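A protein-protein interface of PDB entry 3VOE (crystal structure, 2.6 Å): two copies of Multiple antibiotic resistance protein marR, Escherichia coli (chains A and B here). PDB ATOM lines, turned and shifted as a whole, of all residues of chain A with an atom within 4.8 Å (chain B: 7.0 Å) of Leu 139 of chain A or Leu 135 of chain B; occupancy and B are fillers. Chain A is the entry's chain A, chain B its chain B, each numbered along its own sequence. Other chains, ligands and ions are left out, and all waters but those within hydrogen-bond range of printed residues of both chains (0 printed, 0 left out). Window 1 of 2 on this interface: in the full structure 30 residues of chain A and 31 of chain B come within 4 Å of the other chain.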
ATOM      1  N   LEU A  14     -21.290 -22.103 -16.075  1.00  0.00           N
ATOM      2  CA  LEU A  14     -19.954 -22.674 -16.243  1.00  0.00           C
ATOM      3  C   LEU A  14     -19.951 -24.203 -16.129  1.00  0.00           C
ATOM      4  O   LEU A  14     -19.337 -24.896 -16.947  1.00  0.00           O
ATOM      5  CB  LEU A  14     -18.987 -22.069 -15.219  1.00  0.00           C
ATOM      6  CG  LEU A  14     -17.497 -22.314 -15.465  1.00  0.00           C
ATOM      7  CD1 LEU A  14     -17.032 -21.590 -16.721  1.00  0.00           C
ATOM      8  CD2 LEU A  14     -16.667 -21.897 -14.263  1.00  0.00           C
ATOM      9  N   LEU A 135      -8.608 -18.050 -23.053  1.00  0.00           N
ATOM     10  CA  LEU A 135      -9.389 -19.198 -22.597  1.00  0.00           C
ATOM     11  C   LEU A 135      -8.579 -20.103 -21.666  1.00  0.00           C
ATOM     12  O   LEU A 135      -9.061 -20.503 -20.606  1.00  0.00           O
ATOM     13  CB  LEU A 135      -9.916 -19.995 -23.783  1.00  0.00           C
ATOM     14  CG  LEU A 135     -10.769 -21.232 -23.462  1.00  0.00           C
ATOM     15  CD1 LEU A 135     -11.872 -20.920 -22.446  1.00  0.00           C
ATOM     16  CD2 LEU A 135     -11.356 -21.805 -24.739  1.00  0.00           C
ATOM     17  N   GLU A 136      -7.347 -20.410 -22.064  1.00  0.00           N
ATOM     18  CA  GLU A 136      -6.470 -21.262 -21.261  1.00  0.00           C
ATOM     19  C   GLU A 136      -6.104 -20.617 -19.941  1.00  0.00           C
ATOM     20  O   GLU A 136      -6.035 -21.289 -18.915  1.00  0.00           O
ATOM     21  CB  GLU A 136      -5.213 -21.609 -22.029  1.00  0.00           C
ATOM     22  CG  GLU A 136      -5.395 -22.743 -23.020  1.00  0.00           C
ATOM     23  CD  GLU A 136      -4.246 -22.853 -23.991  1.00  0.00           C
ATOM     24  OE1 GLU A 136      -3.312 -22.020 -23.910  1.00  0.00           O
ATOM     25  OE2 GLU A 136      -4.273 -23.770 -24.837  1.00  0.00           O
ATOM     26  N   TYR A 137      -5.872 -19.309 -19.970  1.00  0.00           N
ATOM     27  CA  TYR A 137      -5.506 -18.566 -18.771  1.00  0.00           C
ATOM     28  C   TYR A 137      -6.631 -18.601 -17.709  1.00  0.00           C
ATOM     29  O   TYR A 137      -6.366 -18.751 -16.507  1.00  0.00           O
ATOM     30  CB  TYR A 137      -5.149 -17.120 -19.136  1.00  0.00           C
ATOM     31  CG  TYR A 137      -5.024 -16.190 -17.945  1.00  0.00           C
ATOM     32  CD1 TYR A 137      -3.915 -16.251 -17.100  1.00  0.00           C
ATOM     33  CD2 TYR A 137      -6.008 -15.241 -17.674  1.00  0.00           C
ATOM     34  CE1 TYR A 137      -3.796 -15.400 -16.013  1.00  0.00           C
ATOM     35  CE2 TYR A 137      -5.895 -14.382 -16.596  1.00  0.00           C
ATOM     36  CZ  TYR A 137      -4.788 -14.467 -15.767  1.00  0.00           C
ATOM     37  OH  TYR A 137      -4.680 -13.623 -14.696  1.00  0.00           O
ATOM     38  N   LEU A 138      -7.876 -18.482 -18.167  1.00  0.00           N
ATOM     39  CA  LEU A 138      -9.023 -18.453 -17.263  1.00  0.00           C
ATOM     40  C   LEU A 138      -9.374 -19.843 -16.744  1.00  0.00           C
ATOM     41  O   LEU A 138      -9.775 -19.996 -15.596  1.00  0.00           O
ATOM     42  CB  LEU A 138     -10.236 -17.810 -17.945  1.00  0.00           C
ATOM     43  CG  LEU A 138     -10.104 -16.317 -18.304  1.00  0.00           C
ATOM     44  CD1 LEU A 138     -11.315 -15.839 -19.095  1.00  0.00           C
ATOM     45  CD2 LEU A 138      -9.907 -15.465 -17.059  1.00  0.00           C
ATOM     46  N   LEU A 139      -9.218 -20.856 -17.595  1.00  0.00           N
ATOM     47  CA  LEU A 139      -9.408 -22.235 -17.167  1.00  0.00           C
ATOM     48  C   LEU A 139      -8.418 -22.610 -16.058  1.00  0.00           C
ATOM     49  O   LEU A 139      -8.805 -23.193 -15.043  1.00  0.00           O
ATOM     50  CB  LEU A 139      -9.278 -23.193 -18.346  1.00  0.00           C
ATOM     51  CG  LEU A 139     -10.422 -23.217 -19.366  1.00  0.00           C
ATOM     52  CD1 LEU A 139     -10.065 -24.118 -20.528  1.00  0.00           C
ATOM     53  CD2 LEU A 139     -11.729 -23.667 -18.730  1.00  0.00           C
ATOM     54  N   LYS A 140      -7.145 -22.241 -16.249  1.00  0.00           N
ATOM     55  CA  LYS A 140      -6.104 -22.459 -15.235  1.00  0.00           C
ATOM     56  C   LYS A 140      -6.518 -21.884 -13.877  1.00  0.00           C
ATOM     57  O   LYS A 140      -6.300 -22.508 -12.845  1.00  0.00           O
ATOM     58  CB  LYS A 140      -4.781 -21.825 -15.676  1.00  0.00           C
ATOM     59  CG  LYS A 140      -4.044 -22.573 -16.779  1.00  0.00           C
ATOM     60  CD  LYS A 140      -2.537 -22.369 -16.657  1.00  0.00           C
ATOM     61  CE  LYS A 140      -1.859 -22.408 -18.017  1.00  0.00           C
ATOM     62  NZ  LYS A 140      -1.809 -21.057 -18.657  1.00  0.00           N
ATOM     63  N   LYS A 141      -7.124 -20.691 -13.898  1.00  0.00           N
ATOM     64  CA  LYS A 141      -7.547 -19.993 -12.673  1.00  0.00           C
ATOM     65  C   LYS A 141      -8.556 -20.786 -11.858  1.00  0.00           C
ATOM     66  O   LYS A 141      -8.661 -20.607 -10.650  1.00  0.00           O
ATOM     67  CB  LYS A 141      -8.126 -18.619 -13.010  1.00  0.00           C
ATOM     68  CG  LYS A 141      -7.080 -17.564 -13.302  1.00  0.00           C
ATOM     69  CD  LYS A 141      -7.608 -16.169 -13.029  1.00  0.00           C
ATOM     70  CE  LYS A 141      -6.504 -15.268 -12.500  1.00  0.00           C
ATOM     71  NZ  LYS A 141      -6.803 -13.824 -12.721  1.00  0.00           N
ATOM     72  N   VAL A 142      -9.304 -21.652 -12.528  1.00  0.00           N
ATOM     73  CA  VAL A 142     -10.350 -22.439 -11.873  1.00  0.00           C
ATOM     74  C   VAL A 142      -9.765 -23.615 -11.067  1.00  0.00           C
ATOM     75  O   VAL A 142     -10.436 -24.173 -10.197  1.00  0.00           O
ATOM     76  CB  VAL A 142     -11.390 -22.969 -12.903  1.00  0.00           C
ATOM     77  CG1 VAL A 142     -12.339 -23.967 -12.256  1.00  0.00           C
ATOM     78  CG2 VAL A 142     -12.169 -21.825 -13.506  1.00  0.00           C
ATOM     79  N   LEU A 143      -8.503 -23.956 -11.333  1.00  0.00           N
ATOM     80  CA  LEU A 143      -7.945 -25.247 -10.895  1.00  0.00           C
ATOM     81  C   LEU A 143      -7.262 -25.251  -9.506  1.00  0.00           C
ATOM     82  O   LEU A 143      -7.130 -26.314  -8.881  1.00  0.00           O
ATOM     83  CB  LEU A 143      -7.010 -25.815 -11.954  1.00  0.00           C
ATOM     84  CG  LEU A 143      -7.729 -26.379 -13.171  1.00  0.00           C
ATOM     85  CD1 LEU A 143      -6.745 -26.677 -14.297  1.00  0.00           C
ATOM     86  CD2 LEU A 143      -8.521 -27.621 -12.785  1.00  0.00           C
ATOM     87  N   PRO B  13      -2.197 -27.516 -22.559  1.00  0.00           N
ATOM     88  CA  PRO B  13      -3.112 -27.559 -23.709  1.00  0.00           C
ATOM     89  C   PRO B  13      -4.579 -27.496 -23.299  1.00  0.00           C
ATOM     90  O   PRO B  13      -4.951 -28.002 -22.238  1.00  0.00           O
ATOM     91  CB  PRO B  13      -2.806 -28.922 -24.349  1.00  0.00           C
ATOM     92  CG  PRO B  13      -1.436 -29.258 -23.886  1.00  0.00           C
ATOM     93  CD  PRO B  13      -1.339 -28.710 -22.502  1.00  0.00           C
ATOM     94  N   LEU B  14      -5.402 -26.900 -24.157  1.00  0.00           N
ATOM     95  CA  LEU B  14      -6.820 -26.682 -23.873  1.00  0.00           C
ATOM     96  C   LEU B  14      -7.549 -27.962 -23.454  1.00  0.00           C
ATOM     97  O   LEU B  14      -8.272 -27.977 -22.455  1.00  0.00           O
ATOM     98  CB  LEU B  14      -7.510 -26.067 -25.087  1.00  0.00           C
ATOM     99  CG  LEU B  14      -8.936 -25.564 -24.878  1.00  0.00           C
ATOM    100  CD1 LEU B  14      -8.972 -24.474 -23.821  1.00  0.00           C
ATOM    101  CD2 LEU B  14      -9.522 -25.064 -26.183  1.00  0.00           C
ATOM    102  N   GLY B  15      -7.369 -29.024 -24.236  1.00  0.00           N
ATOM    103  CA  GLY B  15      -8.040 -30.298 -23.983  1.00  0.00           C
ATOM    104  C   GLY B  15      -7.813 -30.815 -22.576  1.00  0.00           C
ATOM    105  O   GLY B  15      -8.748 -31.255 -21.909  1.00  0.00           O
ATOM    106  N   LEU B  17      -6.801 -28.995 -19.949  1.00  0.00           N
ATOM    107  CA  LEU B  17      -7.389 -28.040 -19.020  1.00  0.00           C
ATOM    108  C   LEU B  17      -8.864 -28.303 -18.824  1.00  0.00           C
ATOM    109  O   LEU B  17      -9.352 -28.334 -17.695  1.00  0.00           O
ATOM    110  CB  LEU B  17      -7.175 -26.610 -19.504  1.00  0.00           C
ATOM    111  CG  LEU B  17      -5.792 -26.015 -19.260  1.00  0.00           C
ATOM    112  CD1 LEU B  17      -5.739 -24.583 -19.770  1.00  0.00           C
ATOM    113  CD2 LEU B  17      -5.424 -26.082 -17.782  1.00  0.00           C
ATOM    114  N   ILE B  18      -9.576 -28.500 -19.925  1.00  0.00           N
ATOM    115  CA  ILE B  18     -10.992 -28.815 -19.862  1.00  0.00           C
ATOM    116  C   ILE B  18     -11.242 -30.106 -19.084  1.00  0.00           C
ATOM    117  O   ILE B  18     -12.180 -30.184 -18.298  1.00  0.00           O
ATOM    118  CB  ILE B  18     -11.628 -28.891 -21.271  1.00  0.00           C
ATOM    119  CG1 ILE B  18     -11.940 -27.483 -21.779  1.00  0.00           C
ATOM    120  CG2 ILE B  18     -12.907 -29.719 -21.245  1.00  0.00           C
ATOM    121  CD1 ILE B  18     -11.809 -27.335 -23.275  1.00  0.00           C
ATOM    122  N   VAL B  21     -10.598 -29.295 -15.295  1.00  0.00           N
ATOM    123  CA  VAL B  21     -11.685 -28.455 -14.784  1.00  0.00           C
ATOM    124  C   VAL B  21     -13.017 -29.213 -14.718  1.00  0.00           C
ATOM    125  O   VAL B  21     -13.825 -28.982 -13.818  1.00  0.00           O
ATOM    126  CB  VAL B  21     -11.848 -27.158 -15.608  1.00  0.00           C
ATOM    127  CG1 VAL B  21     -13.046 -26.363 -15.119  1.00  0.00           C
ATOM    128  CG2 VAL B  21     -10.585 -26.311 -15.522  1.00  0.00           C
ATOM    129  N   LEU B 123     -16.627 -23.017  -8.077  1.00  0.00           N
ATOM    130  CA  LEU B 123     -15.784 -23.062  -9.282  1.00  0.00           C
ATOM    131  C   LEU B 123     -15.192 -21.692  -9.629  1.00  0.00           C
ATOM    132  O   LEU B 123     -14.051 -21.602 -10.075  1.00  0.00           O
ATOM    133  CB  LEU B 123     -16.571 -23.600 -10.478  1.00  0.00           C
ATOM    134  CG  LEU B 123     -16.730 -25.118 -10.599  1.00  0.00           C
ATOM    135  CD1 LEU B 123     -17.514 -25.465 -11.859  1.00  0.00           C
ATOM    136  CD2 LEU B 123     -15.371 -25.814 -10.600  1.00  0.00           C
ATOM    137  N   THR B 124     -15.975 -20.633  -9.406  1.00  0.00           N
ATOM    138  CA  THR B 124     -15.602 -19.285  -9.844  1.00  0.00           C
ATOM    139  C   THR B 124     -15.131 -18.383  -8.689  1.00  0.00           C
ATOM    140  O   THR B 124     -15.211 -17.158  -8.781  1.00  0.00           O
ATOM    141  CB  THR B 124     -16.774 -18.581 -10.568  1.00  0.00           C
ATOM    142  OG1 THR B 124     -17.862 -18.384  -9.652  1.00  0.00           O
ATOM    143  CG2 THR B 124     -17.251 -19.408 -11.755  1.00  0.00           C
ATOM    144  N   LEU B 127     -12.064 -16.146  -9.581  1.00  0.00           N
ATOM    145  CA  LEU B 127     -12.281 -15.314 -10.759  1.00  0.00           C
ATOM    146  C   LEU B 127     -13.194 -14.143 -10.454  1.00  0.00           C
ATOM    147  O   LEU B 127     -14.127 -14.261  -9.655  1.00  0.00           O
ATOM    148  CB  LEU B 127     -12.886 -16.148 -11.892  1.00  0.00           C
ATOM    149  CG  LEU B 127     -11.986 -17.193 -12.548  1.00  0.00           C
ATOM    150  CD1 LEU B 127     -12.819 -18.334 -13.084  1.00  0.00           C
ATOM    151  CD2 LEU B 127     -11.160 -16.571 -13.659  1.00  0.00           C
ATOM    152  N   ASP B 130     -16.228 -10.380 -13.921  1.00  0.00           N
ATOM    153  CA  ASP B 130     -15.705  -9.911 -15.189  1.00  0.00           C
ATOM    154  C   ASP B 130     -15.088 -11.068 -15.973  1.00  0.00           C
ATOM    155  O   ASP B 130     -15.423 -11.292 -17.138  1.00  0.00           O
ATOM    156  CB  ASP B 130     -14.648  -8.831 -14.945  1.00  0.00           C
ATOM    157  CG  ASP B 130     -14.791  -7.659 -15.874  1.00  0.00           C
ATOM    158  OD1 ASP B 130     -15.842  -7.553 -16.547  1.00  0.00           O
ATOM    159  OD2 ASP B 130     -13.861  -6.828 -15.924  1.00  0.00           O
ATOM    160  N   GLU B 131     -14.196 -11.810 -15.314  1.00  0.00           N
ATOM    161  CA  GLU B 131     -13.490 -12.923 -15.948  1.00  0.00           C
ATOM    162  C   GLU B 131     -14.408 -14.111 -16.169  1.00  0.00           C
ATOM    163  O   GLU B 131     -14.262 -14.838 -17.142  1.00  0.00           O
ATOM    164  CB  GLU B 131     -12.292 -13.348 -15.104  1.00  0.00           C
ATOM    165  CG  GLU B 131     -11.150 -12.346 -15.082  1.00  0.00           C
ATOM    166  CD  GLU B 131     -10.178 -12.598 -13.943  1.00  0.00           C
ATOM    167  OE1 GLU B 131      -8.968 -12.711 -14.212  1.00  0.00           O
ATOM    168  OE2 GLU B 131     -10.627 -12.691 -12.781  1.00  0.00           O
ATOM    169  N   VAL B 132     -15.356 -14.307 -15.253  1.00  0.00           N
ATOM    170  CA  VAL B 132     -16.347 -15.377 -15.393  1.00  0.00           C
ATOM    171  C   VAL B 132     -17.103 -15.247 -16.714  1.00  0.00           C
ATOM    172  O   VAL B 132     -17.357 -16.241 -17.394  1.00  0.00           O
ATOM    173  CB  VAL B 132     -17.359 -15.382 -14.222  1.00  0.00           C
ATOM    174  CG1 VAL B 132     -18.485 -16.363 -14.495  1.00  0.00           C
ATOM    175  CG2 VAL B 132     -16.664 -15.731 -12.916  1.00  0.00           C
ATOM    176  N   ALA B 133     -17.441 -14.015 -17.079  1.00  0.00           N
ATOM    177  CA  ALA B 133     -18.210 -13.755 -18.284  1.00  0.00           C
ATOM    178  C   ALA B 133     -17.391 -14.066 -19.522  1.00  0.00           C
ATOM    179  O   ALA B 133     -17.873 -14.715 -20.443  1.00  0.00           O
ATOM    180  CB  ALA B 133     -18.692 -12.310 -18.307  1.00  0.00           C
ATOM    181  N   THR B 134     -16.138 -13.619 -19.524  1.00  0.00           N
ATOM    182  CA  THR B 134     -15.214 -13.914 -20.620  1.00  0.00           C
ATOM    183  C   THR B 134     -15.089 -15.424 -20.815  1.00  0.00           C
ATOM    184  O   THR B 134     -15.197 -15.930 -21.938  1.00  0.00           O
ATOM    185  CB  THR B 134     -13.804 -13.319 -20.355  1.00  0.00           C
ATOM    186  OG1 THR B 134     -13.926 -11.988 -19.840  1.00  0.00           O
ATOM    187  CG2 THR B 134     -12.987 -13.287 -21.630  1.00  0.00           C
ATOM    188  N   LEU B 135     -14.868 -16.140 -19.709  1.00  0.00           N
ATOM    189  CA  LEU B 135     -14.721 -17.593 -19.737  1.00  0.00           C
ATOM    190  C   LEU B 135     -15.950 -18.280 -20.345  1.00  0.00           C
ATOM    191  O   LEU B 135     -15.822 -19.110 -21.251  1.00  0.00           O
ATOM    192  CB  LEU B 135     -14.452 -18.127 -18.330  1.00  0.00           C
ATOM    193  CG  LEU B 135     -14.190 -19.628 -18.170  1.00  0.00           C
ATOM    194  CD1 LEU B 135     -13.048 -20.089 -19.068  1.00  0.00           C
ATOM    195  CD2 LEU B 135     -13.892 -19.954 -16.711  1.00  0.00           C
ATOM    196  N   GLU B 136     -17.135 -17.920 -19.854  1.00  0.00           N
ATOM    197  CA  GLU B 136     -18.388 -18.445 -20.408  1.00  0.00           C
ATOM    198  C   GLU B 136     -18.520 -18.128 -21.902  1.00  0.00           C
ATOM    199  O   GLU B 136     -18.869 -18.996 -22.701  1.00  0.00           O
ATOM    200  CB  GLU B 136     -19.590 -17.896 -19.637  1.00  0.00           C
ATOM    201  CG  GLU B 136     -19.911 -18.673 -18.363  1.00  0.00           C
ATOM    202  CD  GLU B 136     -20.882 -17.940 -17.448  1.00  0.00           C
ATOM    203  OE1 GLU B 136     -21.673 -17.102 -17.945  1.00  0.00           O
ATOM    204  OE2 GLU B 136     -20.859 -18.212 -16.227  1.00  0.00           O
ATOM    205  N   TYR B 137     -18.195 -16.889 -22.266  1.00  0.00           N
ATOM    206  CA  TYR B 137     -18.243 -16.437 -23.655  1.00  0.00           C
ATOM    207  C   TYR B 137     -17.360 -17.294 -24.584  1.00  0.00           C
ATOM    208  O   TYR B 137     -17.795 -17.710 -25.666  1.00  0.00           O
ATOM    209  CB  TYR B 137     -17.831 -14.958 -23.742  1.00  0.00           C
ATOM    210  CG  TYR B 137     -17.656 -14.444 -25.153  1.00  0.00           C
ATOM    211  CD1 TYR B 137     -18.749 -14.329 -26.014  1.00  0.00           C
ATOM    212  CD2 TYR B 137     -16.401 -14.062 -25.627  1.00  0.00           C
ATOM    213  CE1 TYR B 137     -18.595 -13.863 -27.308  1.00  0.00           C
ATOM    214  CE2 TYR B 137     -16.239 -13.591 -26.921  1.00  0.00           C
ATOM    215  CZ  TYR B 137     -17.341 -13.495 -27.756  1.00  0.00           C
ATOM    216  OH  TYR B 137     -17.191 -13.028 -29.039  1.00  0.00           O
ATOM    217  N   LEU B 138     -16.124 -17.544 -24.158  1.00  0.00           N
ATOM    218  CA  LEU B 138     -15.140 -18.210 -25.006  1.00  0.00           C
ATOM    219  C   LEU B 138     -15.357 -19.716 -25.054  1.00  0.00           C
ATOM    220  O   LEU B 138     -15.043 -20.360 -26.047  1.00  0.00           O
ATOM    221  CB  LEU B 138     -13.721 -17.896 -24.529  1.00  0.00           C
ATOM    222  CG  LEU B 138     -13.274 -16.433 -24.592  1.00  0.00           C
ATOM    223  CD1 LEU B 138     -11.866 -16.290 -24.039  1.00  0.00           C
ATOM    224  CD2 LEU B 138     -13.351 -15.894 -26.014  1.00  0.00           C
ATOM    225  N   LEU B 139     -15.892 -20.273 -23.970  1.00  0.00           N
ATOM    226  CA  LEU B 139     -16.308 -21.677 -23.956  1.00  0.00           C
ATOM    227  C   LEU B 139     -17.477 -21.919 -24.906  1.00  0.00           C
ATOM    228  O   LEU B 139     -17.555 -22.969 -25.549  1.00  0.00           O
ATOM    229  CB  LEU B 139     -16.680 -22.120 -22.542  1.00  0.00           C
ATOM    230  CG  LEU B 139     -15.530 -22.483 -21.601  1.00  0.00           C
ATOM    231  CD1 LEU B 139     -16.063 -22.825 -20.222  1.00  0.00           C
ATOM    232  CD2 LEU B 139     -14.699 -23.636 -22.160  1.00  0.00           C
ATOM    233  N   LYS B 140     -18.388 -20.943 -24.984  1.00  0.00           N
ATOM    234  CA  LYS B 140     -19.480 -20.979 -25.954  1.00  0.00           C
ATOM    235  C   LYS B 140     -18.946 -21.023 -27.384  1.00  0.00           C
ATOM    236  O   LYS B 140     -19.541 -21.652 -28.252  1.00  0.00           O
ATOM    237  CB  LYS B 140     -20.392 -19.764 -25.784  1.00  0.00           C
ATOM    238  CG  LYS B 140     -21.409 -19.888 -24.665  1.00  0.00           C
ATOM    239  CD  LYS B 140     -22.638 -19.042 -24.954  1.00  0.00           C
ATOM    240  CE  LYS B 140     -23.267 -18.531 -23.673  1.00  0.00           C
ATOM    241  NZ  LYS B 140     -22.629 -17.265 -23.203  1.00  0.00           N
ATOM    242  N   LYS B 141     -17.817 -20.350 -27.613  1.00  0.00           N
ATOM    243  CA  LYS B 141     -17.237 -20.235 -28.958  1.00  0.00           C
ATOM    244  C   LYS B 141     -16.697 -21.578 -29.470  1.00  0.00           C
ATOM    245  O   LYS B 141     -16.590 -21.794 -30.679  1.00  0.00           O
ATOM    246  CB  LYS B 141     -16.119 -19.177 -28.978  1.00  0.00           C
ATOM    247  CG  LYS B 141     -16.592 -17.748 -28.747  1.00  0.00           C
ATOM    248  CD  LYS B 141     -17.037 -17.086 -30.041  1.00  0.00           C
ATOM    249  CE  LYS B 141     -15.857 -16.503 -30.804  1.00  0.00           C
ATOM    250  NZ  LYS B 141     -16.301 -15.597 -31.900  1.00  0.00           N
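Leu 139 of chain A touches just these residues of chain B: Leu 14, Leu 17, Val 21 and Leu 135.
Printed residues of chain B within 4 Å of Glu 136 of chain A: Leu 14 and Leu 17.
Of the printed residues of chain B, Leu 135 of chain A touches Leu 14 (3.7 Å), Leu 135 (3.7 Å), Leu 138 (3.8 Å) and Leu 139 (3.9 Å).
Pro 13 of chain B touches none of the printed residues of chain A.
Lys 140 of chain B touches none of the printed residues of chain A.
The nearest residue of chain B that does not touch Leu 139 of chain A is Ile 18 of chain B (4.1 Å).
The nearest residue of chain A that does not touch Leu 135 of chain B is Val 142 of chain A (4.1 Å).
The nearest printed residue of chain B that does not touch Val 142 of chain A is Leu 135 of chain B (4.1 Å).
Leu 14 of chain A touches Leu 135 of chain B, and with the chains exchanged Leu 135 of chain A touches Leu 14 of chain B.
Leu 14 of chain A touches Leu 139 of chain B, and with the chains exchanged Leu 139 of chain A touches Leu 14 of chain B.
Leu 135 of chain A touches its own counterpart, Leu 135 of chain B.
Leu 135 of chain A touches Leu 139 of chain B, and with the chains exchanged Leu 139 of chain A touches Leu 135 of chain B.
8 positions are printed for both chains.
The side-chain carboxylate of Glu 131 of chain B is in salt-bridge range of the side-chain amino group of Lys 141 of chain A (2.9 Å).
The side-chain carboxylate (OE2) of Glu 136 of chain A is in hydrogen-bond range of the backbone NH (N) of Leu 14 of chain B, at 3.4 Å.
Leu 14 of chain A touches Glu 136 of chain B.
Leu 14 of chain A touches Leu 139 of chain B (CD1 to CD1, 3.8 Å).
Leu 135 of chain B touches Leu 135 of chain A.
CD1 of Leu 135 of chain A touches CD2 of Leu 139 of chain B, 3.9 Å away.
CD2 of Leu 138 of chain A touches CD2 of Leu 127 of chain B (3.8 Å).
CD1 of Leu 14 of chain B touches CD1 of Leu 139 of chain A, 3.5 Å away.
CD1 of Leu 139 of chain A touches CB of Leu 17 of chain B (3.95 Å).
Lys 140 of chain A touches Leu 17 of chain B (CG to CD2, 3.9 Å).
Val 21 of chain B touches Val 142 of chain A.
CD2 of Leu 143 of chain A touches N of Val 21 of chain B, at 3.7 Å.
NZ of Lys 141 of chain A lies within hydrogen-bond range of OH of Tyr 137 of chain A, 2.9 Å away.
O of Asp 130 of chain B is in hydrogen-bond range of OG1 of Thr 134 of chain B (3.2 Å).
Printed residues of chain A that touch a printed residue of chain B: Leu 14, Leu 135, Glu 136, Leu 138, Leu 139, Lys 140, Lys 141, Val 142 and Leu 143.
Printed residues of chain B that touch a printed residue of chain A: Leu 14, Leu 17, Val 21, Leu 123, Thr 124, Leu 127, Glu 131, Thr 134, Leu 135, Glu 136, Leu 138 and Leu 139.
Hydrophobic or aromatic side chains of chain B that line the printed part of chain A: Leu 14, Leu 17, Val 21, Leu 123, Leu 127, Leu 135, Leu 138 and Leu 139.
Among the printed residues, 26 pairs touch across the chains.
Among the printed residues, Asp or Glu carboxylates within 4 Å of a Lys or Arg side-chain nitrogen of the other chain: Lys 141 of chain A with Glu 131 of chain B.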
